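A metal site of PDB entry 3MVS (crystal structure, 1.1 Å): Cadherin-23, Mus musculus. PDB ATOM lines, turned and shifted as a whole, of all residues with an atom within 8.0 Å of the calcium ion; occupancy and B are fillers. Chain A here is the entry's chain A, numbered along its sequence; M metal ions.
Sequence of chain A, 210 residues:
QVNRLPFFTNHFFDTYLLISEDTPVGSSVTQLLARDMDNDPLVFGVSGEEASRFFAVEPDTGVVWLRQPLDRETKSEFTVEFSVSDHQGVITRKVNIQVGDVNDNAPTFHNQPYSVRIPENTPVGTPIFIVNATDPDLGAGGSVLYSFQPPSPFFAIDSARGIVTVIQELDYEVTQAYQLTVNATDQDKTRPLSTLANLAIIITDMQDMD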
ATOM      1  N   VAL A   2     -12.084 -15.945 -29.176  1.00  0.00           N
ATOM      2  CA  VAL A   2     -11.713 -14.680 -28.588  1.00  0.00           C
ATOM      3  C   VAL A   2     -12.963 -13.894 -28.156  1.00  0.00           C
ATOM      4  O   VAL A   2     -14.093 -14.198 -28.550  1.00  0.00           O
ATOM      5  CB  VAL A   2     -10.792 -13.821 -29.481  1.00  0.00           C
ATOM      6  CG1 VAL A   2      -9.552 -14.608 -29.890  1.00  0.00           C
ATOM      7  CG2 VAL A   2     -11.524 -13.330 -30.690  1.00  0.00           C
ATOM      8  N   ASN A   3     -12.735 -12.933 -27.282  1.00  0.00           N
ATOM      9  CA  ASN A   3     -13.801 -12.171 -26.699  1.00  0.00           C
ATOM     10  C   ASN A   3     -14.698 -11.464 -27.696  1.00  0.00           C
ATOM     11  O   ASN A   3     -14.225 -10.903 -28.669  1.00  0.00           O
ATOM     12  CB  ASN A   3     -13.230 -11.124 -25.769  1.00  0.00           C
ATOM     13  CG  ASN A   3     -14.277 -10.509 -24.895  1.00  0.00           C
ATOM     14  OD1 ASN A   3     -15.082 -11.228 -24.284  1.00  0.00           O
ATOM     15  ND2 ASN A   3     -14.333  -9.189 -24.864  1.00  0.00           N
ATOM     16  N   ARG A   4     -15.999 -11.511 -27.426  1.00  0.00           N
ATOM     17  CA  ARG A   4     -16.963 -10.609 -28.043  1.00  0.00           C
ATOM     18  C   ARG A   4     -17.467  -9.651 -26.983  1.00  0.00           C
ATOM     19  O   ARG A   4     -17.674 -10.044 -25.839  1.00  0.00           O
ATOM     20  CB  ARG A   4     -18.167 -11.373 -28.599  1.00  0.00           C
ATOM     21  CG  ARG A   4     -17.941 -12.061 -29.925  1.00  0.00           C
ATOM     22  CD  ARG A   4     -16.997 -13.252 -29.840  1.00  0.00           C
ATOM     23  NE  ARG A   4     -17.380 -14.225 -28.814  1.00  0.00           N
ATOM     24  CZ  ARG A   4     -18.296 -15.175 -28.965  1.00  0.00           C
ATOM     25  NH1 ARG A   4     -18.948 -15.310 -30.113  1.00  0.00           N
ATOM     26  NH2 ARG A   4     -18.553 -16.017 -27.958  1.00  0.00           N
ATOM     27  N   LEU A   5     -17.718  -8.422 -27.384  1.00  0.00           N
ATOM     28  CA  LEU A   5     -18.303  -7.473 -26.455  1.00  0.00           C
ATOM     29  C   LEU A   5     -19.789  -7.752 -26.218  1.00  0.00           C
ATOM     30  O   LEU A   5     -20.461  -8.358 -27.039  1.00  0.00           O
ATOM     31  CB  LEU A   5     -18.109  -6.058 -26.992  1.00  0.00           C
ATOM     32  CG  LEU A   5     -16.668  -5.538 -27.038  1.00  0.00           C
ATOM     33  CD1 LEU A   5     -16.596  -4.165 -27.702  1.00  0.00           C
ATOM     34  CD2 LEU A   5     -16.058  -5.490 -25.645  1.00  0.00           C
ATOM     35  N   PRO A   6     -20.293  -7.310 -25.076  1.00  0.00           N
ATOM     36  CA  PRO A   6     -21.734  -7.437 -24.849  1.00  0.00           C
ATOM     37  C   PRO A   6     -22.531  -6.532 -25.771  1.00  0.00           C
ATOM     38  O   PRO A   6     -21.979  -5.567 -26.319  1.00  0.00           O
ATOM     39  CB  PRO A   6     -21.897  -6.999 -23.401  1.00  0.00           C
ATOM     40  CG  PRO A   6     -20.682  -6.121 -23.134  1.00  0.00           C
ATOM     41  CD  PRO A   6     -19.585  -6.700 -23.936  1.00  0.00           C
ATOM     42  N   PHE A   7     -23.825  -6.812 -25.919  1.00  0.00           N
ATOM     43  CA  PHE A   7     -24.741  -5.945 -26.647  1.00  0.00           C
ATOM     44  C   PHE A   7     -26.003  -5.739 -25.821  1.00  0.00           C
ATOM     45  O   PHE A   7     -26.458  -6.657 -25.140  1.00  0.00           O
ATOM     46  CB  PHE A   7     -25.067  -6.478 -28.059  1.00  0.00           C
ATOM     47  CG  PHE A   7     -25.636  -7.878 -28.099  1.00  0.00           C
ATOM     48  CD1 PHE A   7     -27.016  -8.112 -28.084  1.00  0.00           C
ATOM     49  CD2 PHE A   7     -24.782  -8.983 -28.219  1.00  0.00           C
ATOM     50  CE1 PHE A   7     -27.540  -9.412 -28.158  1.00  0.00           C
ATOM     51  CE2 PHE A   7     -25.312 -10.291 -28.291  1.00  0.00           C
ATOM     52  CZ  PHE A   7     -26.679 -10.508 -28.264  1.00  0.00           C
ATOM     53  N   ARG A  35     -26.658  -8.994 -23.412  1.00  0.00           N
ATOM     54  CA  ARG A  35     -26.210 -10.366 -23.617  1.00  0.00           C
ATOM     55  C   ARG A  35     -24.724 -10.330 -24.021  1.00  0.00           C
ATOM     56  O   ARG A  35     -24.303  -9.502 -24.827  1.00  0.00           O
ATOM     57  CB  ARG A  35     -27.051 -11.004 -24.741  1.00  0.00           C
ATOM     58  CG  ARG A  35     -26.673 -12.446 -25.099  1.00  0.00           C
ATOM     59  CD  ARG A  35     -27.090 -13.466 -24.053  1.00  0.00           C
ATOM     60  NE  ARG A  35     -26.715 -14.817 -24.491  1.00  0.00           N
ATOM     61  CZ  ARG A  35     -25.794 -15.584 -23.915  1.00  0.00           C
ATOM     62  NH1 ARG A  35     -25.157 -15.189 -22.829  1.00  0.00           N
ATOM     63  NH2 ARG A  35     -25.545 -16.784 -24.428  1.00  0.00           N
ATOM     64  N   ASP A  36     -23.959 -11.247 -23.452  1.00  0.00           N
ATOM     65  CA  ASP A  36     -22.563 -11.438 -23.815  1.00  0.00           C
ATOM     66  C   ASP A  36     -22.406 -12.889 -24.213  1.00  0.00           C
ATOM     67  O   ASP A  36     -22.630 -13.792 -23.400  1.00  0.00           O
ATOM     68  CB  ASP A  36     -21.650 -11.090 -22.649  1.00  0.00           C
ATOM     69  CG  ASP A  36     -20.186 -11.133 -23.016  1.00  0.00           C
ATOM     70  OD1 ASP A  36     -19.558 -10.051 -23.117  1.00  0.00           O
ATOM     71  OD2 ASP A  36     -19.628 -12.234 -23.189  1.00  0.00           O
ATOM     72  N   MET A  37     -22.004 -13.110 -25.444  1.00  0.00           N
ATOM     73  CA  MET A  37     -21.958 -14.468 -25.997  1.00  0.00           C
ATOM     74  C   MET A  37     -20.873 -15.357 -25.379  1.00  0.00           C
ATOM     75  O   MET A  37     -20.911 -16.559 -25.582  1.00  0.00           O
ATOM     76  CB  MET A  37     -21.857 -14.417 -27.514  1.00  0.00           C
ATOM     77  CG  MET A  37     -23.094 -13.809 -28.175  1.00  0.00           C
ATOM     78  SD  MET A  37     -24.659 -14.639 -27.792  1.00  0.00           S
ATOM     79  CE  MET A  37     -24.465 -16.148 -28.719  1.00  0.00           C
ATOM     80  N   ASP A  38     -19.927 -14.758 -24.653  1.00  0.00           N
ATOM     81  CA  ASP A  38     -18.963 -15.542 -23.886  1.00  0.00           C
ATOM     82  C   ASP A  38     -19.495 -15.883 -22.485  1.00  0.00           C
ATOM     83  O   ASP A  38     -18.808 -16.519 -21.693  1.00  0.00           O
ATOM     84  CB  ASP A  38     -17.644 -14.769 -23.768  1.00  0.00           C
ATOM     85  CG  ASP A  38     -17.195 -14.160 -25.072  1.00  0.00           C
ATOM     86  OD1 ASP A  38     -16.796 -14.904 -25.986  1.00  0.00           O
ATOM     87  OD2 ASP A  38     -17.210 -12.924 -25.184  1.00  0.00           O
ATOM     88  N   ASN A  39     -20.703 -15.399 -22.159  1.00  0.00           N
ATOM     89  CA  ASN A  39     -21.278 -15.557 -20.818  1.00  0.00           C
ATOM     90  C   ASN A  39     -20.492 -14.836 -19.721  1.00  0.00           C
ATOM     91  O   ASN A  39     -20.501 -15.242 -18.555  1.00  0.00           O
ATOM     92  CB  ASN A  39     -21.530 -17.028 -20.451  1.00  0.00           C
ATOM     93  CG  ASN A  39     -22.310 -17.751 -21.527  1.00  0.00           C
ATOM     94  OD1 ASN A  39     -23.304 -17.246 -22.051  1.00  0.00           O
ATOM     95  ND2 ASN A  39     -21.864 -18.945 -21.870  1.00  0.00           N
ATOM     96  N   ASP A  40     -19.811 -13.753 -20.102  1.00  0.00           N
ATOM     97  CA  ASP A  40     -19.031 -12.986 -19.159  1.00  0.00           C
ATOM     98  C   ASP A  40     -19.942 -12.257 -18.180  1.00  0.00           C
ATOM     99  O   ASP A  40     -20.988 -11.734 -18.569  1.00  0.00           O
ATOM    100  CB  ASP A  40     -18.191 -11.938 -19.883  1.00  0.00           C
ATOM    101  CG  ASP A  40     -17.065 -12.523 -20.671  1.00  0.00           C
ATOM    102  OD1 ASP A  40     -16.448 -13.510 -20.218  1.00  0.00           O
ATOM    103  OD2 ASP A  40     -16.757 -11.970 -21.744  1.00  0.00           O
ATOM    104  N   PRO A  41     -19.493 -12.088 -16.927  1.00  0.00           N
ATOM    105  CA  PRO A  41     -20.148 -11.143 -16.024  1.00  0.00           C
ATOM    106  C   PRO A  41     -20.035  -9.707 -16.553  1.00  0.00           C
ATOM    107  O   PRO A  41     -19.026  -9.312 -17.139  1.00  0.00           O
ATOM    108  CB  PRO A  41     -19.355 -11.294 -14.710  1.00  0.00           C
ATOM    109  CG  PRO A  41     -18.610 -12.556 -14.823  1.00  0.00           C
ATOM    110  CD  PRO A  41     -18.344 -12.760 -16.278  1.00  0.00           C
ATOM    111  N   LEU A  42     -21.092  -8.948 -16.325  1.00  0.00           N
ATOM    112  CA  LEU A  42     -21.236  -7.624 -16.925  1.00  0.00           C
ATOM    113  C   LEU A  42     -21.286  -6.522 -15.905  1.00  0.00           C
ATOM    114  O   LEU A  42     -21.696  -6.736 -14.757  1.00  0.00           O
ATOM    115  CB  LEU A  42     -22.506  -7.567 -17.756  1.00  0.00           C
ATOM    116  CG  LEU A  42     -22.571  -8.602 -18.885  1.00  0.00           C
ATOM    117  CD1 LEU A  42     -23.829  -8.415 -19.693  1.00  0.00           C
ATOM    118  CD2 LEU A  42     -21.331  -8.496 -19.784  1.00  0.00           C
ATOM    119  N   SER A  85     -20.115  -3.408 -20.006  1.00  0.00           N
ATOM    120  CA  SER A  85     -18.772  -3.961 -20.131  1.00  0.00           C
ATOM    121  C   SER A  85     -18.747  -5.401 -19.650  1.00  0.00           C
ATOM    122  O   SER A  85     -19.484  -5.773 -18.743  1.00  0.00           O
ATOM    123  CB  SER A  85     -17.803  -3.148 -19.243  1.00  0.00           C
ATOM    124  OG  SER A  85     -16.515  -3.759 -19.167  1.00  0.00           O
ATOM    125  N   ASP A  86     -17.862  -6.187 -20.259  1.00  0.00           N
ATOM    126  CA  ASP A  86     -17.585  -7.552 -19.817  1.00  0.00           C
ATOM    127  C   ASP A  86     -16.266  -7.677 -19.059  1.00  0.00           C
ATOM    128  O   ASP A  86     -15.677  -8.760 -19.014  1.00  0.00           O
ATOM    129  CB  ASP A  86     -17.602  -8.496 -21.028  1.00  0.00           C
ATOM    130  CG  ASP A  86     -16.582  -8.121 -22.089  1.00  0.00           C
ATOM    131  OD1 ASP A  86     -15.803  -7.166 -21.876  1.00  0.00           O
ATOM    132  OD2 ASP A  86     -16.546  -8.833 -23.113  1.00  0.00           O
ATOM    133  N   HIS A  87     -15.791  -6.562 -18.503  1.00  0.00           N
ATOM    134  CA  HIS A  87     -14.480  -6.467 -17.789  1.00  0.00           C
ATOM    135  C   HIS A  87     -13.269  -6.466 -18.713  1.00  0.00           C
ATOM    136  O   HIS A  87     -12.147  -6.332 -18.252  1.00  0.00           O
ATOM    137  CB  HIS A  87     -14.311  -7.535 -16.690  1.00  0.00           C
ATOM    138  CG  HIS A  87     -15.301  -7.421 -15.582  1.00  0.00           C
ATOM    139  ND1 HIS A  87     -15.117  -6.576 -14.516  1.00  0.00           N
ATOM    140  CD2 HIS A  87     -16.493  -8.021 -15.380  1.00  0.00           C
ATOM    141  CE1 HIS A  87     -16.140  -6.695 -13.681  1.00  0.00           C
ATOM    142  NE2 HIS A  87     -16.990  -7.554 -14.192  1.00  0.00           N
ATOM    143  N   GLN A  88     -13.499  -6.596 -20.006  1.00  0.00           N
ATOM    144  CA  GLN A  88     -12.442  -6.548 -21.014  1.00  0.00           C
ATOM    145  C   GLN A  88     -12.556  -5.289 -21.864  1.00  0.00           C
ATOM    146  O   GLN A  88     -11.592  -4.531 -21.980  1.00  0.00           O
ATOM    147  CB  GLN A  88     -12.484  -7.797 -21.872  1.00  0.00           C
ATOM    148  CG  GLN A  88     -12.232  -9.044 -21.036  1.00  0.00           C
ATOM    149  CD  GLN A  88     -12.887 -10.258 -21.625  1.00  0.00           C
ATOM    150  OE1 GLN A  88     -12.272 -10.923 -22.478  1.00  0.00           O
ATOM    151  NE2 GLN A  88     -14.147 -10.562 -21.216  1.00  0.00           N
ATOM    152  N   GLY A  89     -13.741  -5.088 -22.449  1.00  0.00           N
ATOM    153  CA  GLY A  89     -14.063  -3.862 -23.167  1.00  0.00           C
ATOM    154  C   GLY A  89     -15.394  -3.327 -22.728  1.00  0.00           C
ATOM    155  O   GLY A  89     -16.037  -3.863 -21.822  1.00  0.00           O
HETATM  156 CA    CA M   1     -17.420 -10.985 -23.782  1.00  0.00          CA
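The backbone carbonyl oxygen (O) of Met 37 sits at hydrogen-bond distance from the guanidinium group (NH2) of Arg 4. The side-chain amide oxygen (OD1) of Asn 3 lies close to the side-chain amide nitrogen (NE2) of Gln 88 (3.3 Å). The side-chain carboxylate of Asp 36 lies close to the backbone NH of Asn 39. NE of Arg 4 is in hydrogen-bond range of O of Val 2, 3.3 Å away. The side-chain carboxylate (OD1) of Asp 86 is in hydrogen-bond range of the backbone NH (N) of Gln 88 (3.0 Å). OD2 of Asp 40 lies close to NE2 of Gln 88, 3.0 Å away. The side-chain carboxylate of Asp 86 sits at hydrogen-bond distance from the backbone NH of Gly 89 (3.0 Å).
The calcium ion is bound by O of Arg 4 (2.3 Å), OD2 of Asp 40 (2.4 Å), OD2 of Asp 38 (2.4 Å), OD1 of Asn 3 (2.4 Å), OD2 of Asp 86 (2.4 Å), OD1 of Asp 36 (2.4 Å) and OD2 of Asp 36 (2.6 Å).
Within 4 Å of the calcium ion: Asn 3, Arg 4, Asp 36, Asp 38, Asp 40 and Asp 86.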
